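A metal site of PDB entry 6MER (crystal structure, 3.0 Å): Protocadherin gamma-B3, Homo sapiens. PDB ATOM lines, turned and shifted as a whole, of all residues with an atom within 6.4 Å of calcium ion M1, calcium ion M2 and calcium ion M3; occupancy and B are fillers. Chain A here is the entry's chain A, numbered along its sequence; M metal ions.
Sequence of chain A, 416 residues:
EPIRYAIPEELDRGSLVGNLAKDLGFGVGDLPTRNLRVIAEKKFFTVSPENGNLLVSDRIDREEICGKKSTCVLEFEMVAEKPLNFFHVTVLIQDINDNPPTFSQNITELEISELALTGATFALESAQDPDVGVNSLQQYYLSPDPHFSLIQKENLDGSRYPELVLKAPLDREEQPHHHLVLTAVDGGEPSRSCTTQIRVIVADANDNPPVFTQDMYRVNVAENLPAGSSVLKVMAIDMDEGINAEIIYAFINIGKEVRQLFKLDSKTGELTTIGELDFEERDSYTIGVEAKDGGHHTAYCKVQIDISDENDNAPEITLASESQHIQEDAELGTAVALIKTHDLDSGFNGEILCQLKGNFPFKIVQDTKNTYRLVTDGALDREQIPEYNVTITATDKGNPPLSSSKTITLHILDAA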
ATOM      1  N   GLU A   9       5.638 -24.995   2.921  1.00  0.00           N
ATOM      2  CA  GLU A   9       4.893 -24.736   4.140  1.00  0.00           C
ATOM      3  C   GLU A   9       3.444 -25.193   4.006  1.00  0.00           C
ATOM      4  O   GLU A   9       2.990 -25.591   2.935  1.00  0.00           O
ATOM      5  CB  GLU A   9       4.941 -23.247   4.490  1.00  0.00           C
ATOM      6  CG  GLU A   9       4.416 -22.347   3.393  1.00  0.00           C
ATOM      7  CD  GLU A   9       4.002 -20.981   3.907  1.00  0.00           C
ATOM      8  OE1 GLU A   9       3.779 -20.846   5.127  1.00  0.00           O
ATOM      9  OE2 GLU A   9       3.911 -20.044   3.089  1.00  0.00           O
ATOM     10  N   GLU A  10       2.723 -25.133   5.122  1.00  0.00           N
ATOM     11  CA  GLU A  10       1.298 -25.442   5.175  1.00  0.00           C
ATOM     12  C   GLU A  10       1.016 -26.873   4.704  1.00  0.00           C
ATOM     13  O   GLU A  10       0.107 -27.121   3.910  1.00  0.00           O
ATOM     14  CB  GLU A  10       0.486 -24.423   4.373  1.00  0.00           C
ATOM     15  CG  GLU A  10       0.727 -22.973   4.755  1.00  0.00           C
ATOM     16  CD  GLU A  10       0.136 -22.602   6.095  1.00  0.00           C
ATOM     17  OE1 GLU A  10      -0.586 -23.428   6.691  1.00  0.00           O
ATOM     18  OE2 GLU A  10       0.382 -21.469   6.566  1.00  0.00           O
ATOM     19  N   ARG A  59       0.882 -27.069  12.293  1.00  0.00           N
ATOM     20  CA  ARG A  59       0.810 -26.208  11.122  1.00  0.00           C
ATOM     21  C   ARG A  59       2.106 -25.425  10.947  1.00  0.00           C
ATOM     22  O   ARG A  59       2.583 -24.776  11.892  1.00  0.00           O
ATOM     23  CB  ARG A  59      -0.377 -25.249  11.248  1.00  0.00           C
ATOM     24  CG  ARG A  59      -0.515 -24.262  10.099  1.00  0.00           C
ATOM     25  CD  ARG A  59      -1.797 -23.457  10.216  1.00  0.00           C
ATOM     26  NE  ARG A  59      -1.924 -22.462   9.161  1.00  0.00           N
ATOM     27  CZ  ARG A  59      -1.615 -21.178   9.301  1.00  0.00           C
ATOM     28  NH1 ARG A  59      -1.150 -20.721  10.461  1.00  0.00           N
ATOM     29  NH2 ARG A  59      -1.770 -20.340   8.282  1.00  0.00           N
ATOM     30  N   ILE A  60       2.672 -25.485   9.755  1.00  0.00           N
ATOM     31  CA  ILE A  60       3.936 -24.817   9.441  1.00  0.00           C
ATOM     32  C   ILE A  60       3.585 -23.564   8.654  1.00  0.00           C
ATOM     33  O   ILE A  60       3.484 -23.584   7.419  1.00  0.00           O
ATOM     34  CB  ILE A  60       4.897 -25.731   8.683  1.00  0.00           C
ATOM     35  CG1 ILE A  60       5.053 -27.068   9.416  1.00  0.00           C
ATOM     36  CG2 ILE A  60       6.252 -25.062   8.527  1.00  0.00           C
ATOM     37  CD1 ILE A  60       5.616 -26.946  10.814  1.00  0.00           C
ATOM     38  N   ASP A  61       3.397 -22.457   9.360  1.00  0.00           N
ATOM     39  CA  ASP A  61       3.112 -21.167   8.747  1.00  0.00           C
ATOM     40  C   ASP A  61       4.425 -20.387   8.671  1.00  0.00           C
ATOM     41  O   ASP A  61       4.996 -20.022   9.702  1.00  0.00           O
ATOM     42  CB  ASP A  61       2.058 -20.398   9.541  1.00  0.00           C
ATOM     43  CG  ASP A  61       1.716 -19.055   8.928  1.00  0.00           C
ATOM     44  OD1 ASP A  61       1.007 -19.035   7.892  1.00  0.00           O
ATOM     45  OD2 ASP A  61       2.147 -18.020   9.466  1.00  0.00           O
ATOM     46  N   ARG A  62       4.885 -20.130   7.452  1.00  0.00           N
ATOM     47  CA  ARG A  62       6.170 -19.447   7.282  1.00  0.00           C
ATOM     48  C   ARG A  62       6.101 -17.996   7.734  1.00  0.00           C
ATOM     49  O   ARG A  62       7.122 -17.414   8.126  1.00  0.00           O
ATOM     50  CB  ARG A  62       6.619 -19.524   5.820  1.00  0.00           C
ATOM     51  CG  ARG A  62       8.092 -19.184   5.619  1.00  0.00           C
ATOM     52  CD  ARG A  62       8.326 -18.597   4.234  1.00  0.00           C
ATOM     53  NE  ARG A  62       7.624 -17.336   4.067  1.00  0.00           N
ATOM     54  CZ  ARG A  62       8.094 -16.155   4.454  1.00  0.00           C
ATOM     55  NH1 ARG A  62       9.284 -16.076   5.034  1.00  0.00           N
ATOM     56  NH2 ARG A  62       7.382 -15.056   4.264  1.00  0.00           N
ATOM     57  N   GLU A  63       4.909 -17.383   7.690  1.00  0.00           N
ATOM     58  CA  GLU A  63       4.770 -15.989   8.102  1.00  0.00           C
ATOM     59  C   GLU A  63       4.788 -15.832   9.618  1.00  0.00           C
ATOM     60  O   GLU A  63       5.175 -14.767  10.121  1.00  0.00           O
ATOM     61  CB  GLU A  63       3.480 -15.397   7.531  1.00  0.00           C
ATOM     62  CG  GLU A  63       3.542 -15.081   6.042  1.00  0.00           C
ATOM     63  CD  GLU A  63       3.566 -16.329   5.178  1.00  0.00           C
ATOM     64  OE1 GLU A  63       2.853 -17.299   5.502  1.00  0.00           O
ATOM     65  OE2 GLU A  63       4.292 -16.339   4.160  1.00  0.00           O
ATOM     66  N   GLU A  64       4.389 -16.865  10.350  1.00  0.00           N
ATOM     67  CA  GLU A  64       4.438 -16.804  11.813  1.00  0.00           C
ATOM     68  C   GLU A  64       5.838 -17.072  12.340  1.00  0.00           C
ATOM     69  O   GLU A  64       6.198 -16.595  13.423  1.00  0.00           O
ATOM     70  CB  GLU A  64       3.443 -17.811  12.404  1.00  0.00           C
ATOM     71  CG  GLU A  64       3.351 -17.794  13.924  1.00  0.00           C
ATOM     72  CD  GLU A  64       2.686 -16.542  14.459  1.00  0.00           C
ATOM     73  OE1 GLU A  64       1.984 -15.861  13.688  1.00  0.00           O
ATOM     74  OE2 GLU A  64       2.871 -16.233  15.663  1.00  0.00           O
ATOM     75  N   GLN A  94       9.894 -23.657   2.465  1.00  0.00           N
ATOM     76  CA  GLN A  94       9.695 -22.933   1.222  1.00  0.00           C
ATOM     77  C   GLN A  94       8.399 -22.135   1.276  1.00  0.00           C
ATOM     78  O   GLN A  94       7.399 -22.590   1.845  1.00  0.00           O
ATOM     79  CB  GLN A  94       9.676 -23.896   0.040  1.00  0.00           C
ATOM     80  CG  GLN A  94      10.993 -24.636  -0.166  1.00  0.00           C
ATOM     81  CD  GLN A  94      10.915 -25.670  -1.281  1.00  0.00           C
ATOM     82  OE1 GLN A  94       9.831 -26.148  -1.624  1.00  0.00           O
ATOM     83  NE2 GLN A  94      12.062 -26.009  -1.845  1.00  0.00           N
ATOM     84  N   ASP A  95       8.422 -20.947   0.691  1.00  0.00           N
ATOM     85  CA  ASP A  95       7.284 -20.038   0.724  1.00  0.00           C
ATOM     86  C   ASP A  95       6.317 -20.355  -0.406  1.00  0.00           C
ATOM     87  O   ASP A  95       6.728 -20.486  -1.568  1.00  0.00           O
ATOM     88  CB  ASP A  95       7.749 -18.591   0.623  1.00  0.00           C
ATOM     89  CG  ASP A  95       6.606 -17.599   0.589  1.00  0.00           C
ATOM     90  OD1 ASP A  95       5.960 -17.391   1.638  1.00  0.00           O
ATOM     91  OD2 ASP A  95       6.340 -17.025  -0.494  1.00  0.00           O
ATOM     92  N   ILE A  96       5.034 -20.478  -0.066  1.00  0.00           N
ATOM     93  CA  ILE A  96       3.969 -20.643  -1.057  1.00  0.00           C
ATOM     94  C   ILE A  96       3.111 -19.382  -1.032  1.00  0.00           C
ATOM     95  O   ILE A  96       2.991 -18.707  -0.004  1.00  0.00           O
ATOM     96  CB  ILE A  96       3.112 -21.900  -0.788  1.00  0.00           C
ATOM     97  CG1 ILE A  96       2.326 -21.756   0.511  1.00  0.00           C
ATOM     98  CG2 ILE A  96       3.983 -23.143  -0.763  1.00  0.00           C
ATOM     99  CD1 ILE A  96       1.414 -22.921   0.812  1.00  0.00           C
ATOM    100  N   ASN A  97       2.520 -19.069  -2.183  1.00  0.00           N
ATOM    101  CA  ASN A  97       1.701 -17.867  -2.324  1.00  0.00           C
ATOM    102  C   ASN A  97       0.301 -18.161  -1.800  1.00  0.00           C
ATOM    103  O   ASN A  97      -0.659 -18.388  -2.555  1.00  0.00           O
ATOM    104  CB  ASN A  97       1.672 -17.411  -3.781  1.00  0.00           C
ATOM    105  CG  ASN A  97       0.975 -16.080  -3.953  1.00  0.00           C
ATOM    106  OD1 ASN A  97       0.829 -15.308  -2.991  1.00  0.00           O
ATOM    107  ND2 ASN A  97       0.526 -15.786  -5.166  1.00  0.00           N
ATOM    108  N   ASP A  98       0.179 -18.158  -0.472  1.00  0.00           N
ATOM    109  CA  ASP A  98      -1.085 -18.428   0.194  1.00  0.00           C
ATOM    110  C   ASP A  98      -1.697 -17.186   0.824  1.00  0.00           C
ATOM    111  O   ASP A  98      -2.813 -17.261   1.344  1.00  0.00           O
ATOM    112  CB  ASP A  98      -0.901 -19.506   1.263  1.00  0.00           C
ATOM    113  CG  ASP A  98       0.226 -19.190   2.237  1.00  0.00           C
ATOM    114  OD1 ASP A  98       0.918 -18.165   2.043  1.00  0.00           O
ATOM    115  OD2 ASP A  98       0.412 -19.962   3.199  1.00  0.00           O
ATOM    116  N   ASN A  99      -1.011 -16.048   0.773  1.00  0.00           N
ATOM    117  CA  ASN A  99      -1.519 -14.806   1.331  1.00  0.00           C
ATOM    118  C   ASN A  99      -1.704 -13.779   0.222  1.00  0.00           C
ATOM    119  O   ASN A  99      -0.781 -13.553  -0.576  1.00  0.00           O
ATOM    120  CB  ASN A  99      -0.568 -14.252   2.407  1.00  0.00           C
ATOM    121  CG  ASN A  99      -0.522 -15.129   3.646  1.00  0.00           C
ATOM    122  OD1 ASN A  99       0.500 -15.739   3.953  1.00  0.00           O
ATOM    123  ND2 ASN A  99      -1.634 -15.184   4.367  1.00  0.00           N
ATOM    124  N   PRO A 100      -2.867 -13.141   0.134  1.00  0.00           N
ATOM    125  CA  PRO A 100      -3.083 -12.128  -0.899  1.00  0.00           C
ATOM    126  C   PRO A 100      -2.530 -10.780  -0.454  1.00  0.00           C
ATOM    127  O   PRO A 100      -2.345 -10.543   0.745  1.00  0.00           O
ATOM    128  CB  PRO A 100      -4.603 -12.092  -1.038  1.00  0.00           C
ATOM    129  CG  PRO A 100      -5.090 -12.414   0.342  1.00  0.00           C
ATOM    130  CD  PRO A 100      -4.084 -13.379   0.922  1.00  0.00           C
ATOM    131  N   PRO A 101      -2.263  -9.884  -1.406  1.00  0.00           N
ATOM    132  CA  PRO A 101      -1.845  -8.530  -1.028  1.00  0.00           C
ATOM    133  C   PRO A 101      -2.971  -7.787  -0.324  1.00  0.00           C
ATOM    134  O   PRO A 101      -4.146  -8.125  -0.435  1.00  0.00           O
ATOM    135  CB  PRO A 101      -1.505  -7.872  -2.368  1.00  0.00           C
ATOM    136  CG  PRO A 101      -1.298  -9.003  -3.321  1.00  0.00           C
ATOM    137  CD  PRO A 101      -2.221 -10.085  -2.855  1.00  0.00           C
ATOM    138  N   ASP A 129       2.561  -7.592   1.316  1.00  0.00           N
ATOM    139  CA  ASP A 129       2.361  -9.020   1.086  1.00  0.00           C
ATOM    140  C   ASP A 129       3.164  -9.782   2.139  1.00  0.00           C
ATOM    141  O   ASP A 129       4.397  -9.609   2.205  1.00  0.00           O
ATOM    142  CB  ASP A 129       2.792  -9.420  -0.330  1.00  0.00           C
ATOM    143  CG  ASP A 129       1.976 -10.573  -0.879  1.00  0.00           C
ATOM    144  OD1 ASP A 129       1.423 -11.351  -0.081  1.00  0.00           O
ATOM    145  OD2 ASP A 129       1.891 -10.697  -2.118  1.00  0.00           O
ATOM    146  N   PRO A 130       2.529 -10.605   2.969  1.00  0.00           N
ATOM    147  CA  PRO A 130       3.278 -11.316   4.012  1.00  0.00           C
ATOM    148  C   PRO A 130       4.289 -12.321   3.478  1.00  0.00           C
ATOM    149  O   PRO A 130       5.198 -12.716   4.223  1.00  0.00           O
ATOM    150  CB  PRO A 130       2.184 -12.017   4.827  1.00  0.00           C
ATOM    151  CG  PRO A 130       0.923 -11.277   4.502  1.00  0.00           C
ATOM    152  CD  PRO A 130       1.078 -10.837   3.080  1.00  0.00           C
ATOM    153  N   ASP A 131       4.165 -12.733   2.226  1.00  0.00           N
ATOM    154  CA  ASP A 131       5.083 -13.720   1.655  1.00  0.00           C
ATOM    155  C   ASP A 131       6.398 -13.053   1.266  1.00  0.00           C
ATOM    156  O   ASP A 131       6.599 -11.849   1.451  1.00  0.00           O
ATOM    157  CB  ASP A 131       4.436 -14.406   0.450  1.00  0.00           C
ATOM    158  CG  ASP A 131       3.002 -14.825   0.723  1.00  0.00           C
ATOM    159  OD1 ASP A 131       2.113 -13.956   0.658  1.00  0.00           O
ATOM    160  OD2 ASP A 131       2.775 -16.014   0.994  1.00  0.00           O
ATOM    161  N   VAL A 132       7.318 -13.846   0.723  1.00  0.00           N
ATOM    162  CA  VAL A 132       8.617 -13.369   0.266  1.00  0.00           C
ATOM    163  C   VAL A 132       8.863 -13.875  -1.142  1.00  0.00           C
ATOM    164  O   VAL A 132       8.110 -14.694  -1.681  1.00  0.00           O
ATOM    165  CB  VAL A 132       9.760 -13.801   1.209  1.00  0.00           C
ATOM    166  CG1 VAL A 132       9.601 -13.180   2.581  1.00  0.00           C
ATOM    167  CG2 VAL A 132       9.814 -15.321   1.315  1.00  0.00           C
ATOM    168  N   VAL A 134       9.117 -14.125  -5.157  1.00  0.00           N
ATOM    169  CA  VAL A 134       8.199 -13.758  -6.229  1.00  0.00           C
ATOM    170  C   VAL A 134       6.761 -13.688  -5.737  1.00  0.00           C
ATOM    171  O   VAL A 134       5.935 -13.014  -6.356  1.00  0.00           O
ATOM    172  CB  VAL A 134       8.328 -14.731  -7.414  1.00  0.00           C
ATOM    173  CG1 VAL A 134       9.746 -14.716  -7.969  1.00  0.00           C
ATOM    174  CG2 VAL A 134       7.933 -16.141  -6.991  1.00  0.00           C
ATOM    175  N   ASN A 135       6.438 -14.359  -4.633  1.00  0.00           N
ATOM    176  CA  ASN A 135       5.099 -14.298  -4.069  1.00  0.00           C
ATOM    177  C   ASN A 135       4.818 -12.969  -3.385  1.00  0.00           C
ATOM    178  O   ASN A 135       3.683 -12.754  -2.937  1.00  0.00           O
ATOM    179  CB  ASN A 135       4.893 -15.441  -3.087  1.00  0.00           C
ATOM    180  CG  ASN A 135       5.163 -16.799  -3.695  1.00  0.00           C
ATOM    181  OD1 ASN A 135       4.888 -17.028  -4.872  1.00  0.00           O
ATOM    182  ND2 ASN A 135       5.728 -17.707  -2.902  1.00  0.00           N
ATOM    183  N   SER A 136       5.809 -12.085  -3.283  1.00  0.00           N
ATOM    184  CA  SER A 136       5.632 -10.766  -2.693  1.00  0.00           C
ATOM    185  C   SER A 136       5.788  -9.623  -3.689  1.00  0.00           C
ATOM    186  O   SER A 136       5.298  -8.527  -3.422  1.00  0.00           O
ATOM    187  CB  SER A 136       6.610 -10.553  -1.536  1.00  0.00           C
ATOM    188  OG  SER A 136       6.414  -9.302  -0.914  1.00  0.00           O
ATOM    189  N   GLN A 138       4.847  -7.262  -6.455  1.00  0.00           N
ATOM    190  CA  GLN A 138       3.517  -6.845  -6.861  1.00  0.00           C
ATOM    191  C   GLN A 138       3.529  -6.183  -8.229  1.00  0.00           C
ATOM    192  O   GLN A 138       4.510  -5.541  -8.624  1.00  0.00           O
ATOM    193  CB  GLN A 138       2.910  -5.869  -5.833  1.00  0.00           C
ATOM    194  CG  GLN A 138       2.795  -6.449  -4.434  1.00  0.00           C
ATOM    195  CD  GLN A 138       1.854  -7.629  -4.371  1.00  0.00           C
ATOM    196  OE1 GLN A 138       0.952  -7.775  -5.205  1.00  0.00           O
ATOM    197  NE2 GLN A 138       2.051  -8.485  -3.373  1.00  0.00           N
ATOM    198  N   ASP A 186       0.165 -10.074  -7.118  1.00  0.00           N
ATOM    199  CA  ASP A 186       1.491 -10.623  -6.891  1.00  0.00           C
ATOM    200  C   ASP A 186       1.853 -11.621  -7.982  1.00  0.00           C
ATOM    201  O   ASP A 186       1.014 -12.066  -8.767  1.00  0.00           O
ATOM    202  CB  ASP A 186       1.579 -11.264  -5.509  1.00  0.00           C
ATOM    203  CG  ASP A 186       0.479 -12.279  -5.249  1.00  0.00           C
ATOM    204  OD1 ASP A 186      -0.265 -12.620  -6.200  1.00  0.00           O
ATOM    205  OD2 ASP A 186       0.356 -12.745  -4.101  1.00  0.00           O
ATOM    206  N   ARG A 192      -2.769 -14.029  -6.517  1.00  0.00           N
ATOM    207  CA  ARG A 192      -3.771 -13.414  -5.661  1.00  0.00           C
ATOM    208  C   ARG A 192      -3.781 -11.903  -5.857  1.00  0.00           C
ATOM    209  O   ARG A 192      -2.741 -11.283  -6.108  1.00  0.00           O
ATOM    210  CB  ARG A 192      -3.505 -13.753  -4.198  1.00  0.00           C
ATOM    211  CG  ARG A 192      -3.461 -15.251  -3.930  1.00  0.00           C
ATOM    212  CD  ARG A 192      -3.340 -15.562  -2.440  1.00  0.00           C
ATOM    213  NE  ARG A 192      -3.328 -16.992  -2.195  1.00  0.00           N
ATOM    214  CZ  ARG A 192      -4.419 -17.734  -2.047  1.00  0.00           C
ATOM    215  NH1 ARG A 192      -5.618 -17.180  -2.122  1.00  0.00           N
ATOM    216  NH2 ARG A 192      -4.323 -19.038  -1.828  1.00  0.00           N
HETATM  217 CA    CA M   1       3.569 -17.804   2.355  1.00  0.00          CA
HETATM  218 CA    CA M   2       1.494 -13.269  -1.785  1.00  0.00          CA
HETATM  219 CA    CA M   3       1.259 -19.317   5.447  1.00  0.00          CA
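OE1 of Glu 9 sits at hydrogen-bond distance from N of Arg 62, 2.7 Å away.
The backbone NH (N) of Glu 9 lies within hydrogen-bond range of the backbone carbonyl oxygen (O) of Gln 94, 3.2 Å away.
The side-chain carboxylate (OE2) of Glu 63 lies close to the guanidinium group (NH2) of Arg 62 (3.3 Å).
The guanidinium group (NE) of Arg 192 lies within hydrogen-bond range of the backbone carbonyl oxygen (O) of Asn 97, 3.0 Å away.
OD2 of Asp 61 lies within hydrogen-bond range of N of Glu 64 (2.7 Å).
The side-chain carboxylate (OD2) of Asp 129 sits close to the side-chain amide nitrogen (NE2) of Gln 138, 2.5 Å away.
The side-chain carboxylate (OE1) of Glu 10 lies within salt-bridge range of the guanidinium group (NE) of Arg 59, 3.0 Å away.
The side-chain amide oxygen of Gln 138 sits at hydrogen-bond distance from the backbone NH of Asp 186.
Along chain A the residues within 4 Å of calcium ion M1 span positions 9 to 131.
The nearest printed residue that does not touch calcium ion M1 is Asn 99 (4.03 Å).
Within 4 Å of calcium ion M2: Asn 97, Asn 99, Asp 129, Asp 131, Asn 135 and Asp 186.
Along chain A the residues within 4 Å of calcium ion M2 span positions 97 to 186.
The nearest printed residue that does not touch calcium ion M2 is Ser 136 (4.7 Å).
Six residues have an atom within 4 Å of calcium ion M3: Glu 9, Glu 10, Asp 61, Glu 63, Asp 98 and Asn 99.
The nearest printed residue that does not touch calcium ion M3 is Arg 62 (4.2 Å).
OE2 of Glu 9 binds calcium ion M1 (2.4 Å).
The side-chain carboxylate (OD2) of Asp 131 binds calcium ion M1, at 2.4 Å.
Calcium ion M1 is bound by the side-chain carboxylate (OE2) of Glu 63 (2.4 Å).
OD1 of Asp 95 is bound to calcium ion M1 (2.5 Å).
Calcium ion M1 is bound by O of Ile 96.
Calcium ion M1 is bound by OD1 of Asp 98.
Calcium ion M2 is bound by the side-chain amide oxygen (OD1) of Asn 97 (2.5 Å), the backbone carbonyl oxygen (O) of Asn 135 (2.5 Å), the side-chain carboxylate (OD1) of Asp 129 (2.6 Å), the backbone carbonyl oxygen (O) of Asn 99 (2.6 Å), the side-chain carboxylate (OD1) of Asp 131 (2.6 Å), the side-chain carboxylate (OD2) of Asp 129 (2.6 Å) and the side-chain carboxylate (OD2) of Asp 186 (2.6 Å).
Calcium ion M3 is bound by the side-chain carboxylate (OD1) of Asp 61 (2.5 Å), the side-chain carboxylate (OD2) of Asp 98 (2.5 Å), the side-chain carboxylate (OE1) of Glu 63 (2.6 Å) and the side-chain carboxylate (OE2) of Glu 10 (2.6 Å).
Calcium ion M3 has four donor atoms within binding distance.
Slightly farther from calcium ion M3 lies the side-chain carboxylate (OE1) of Glu 9 (3.0 Å).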
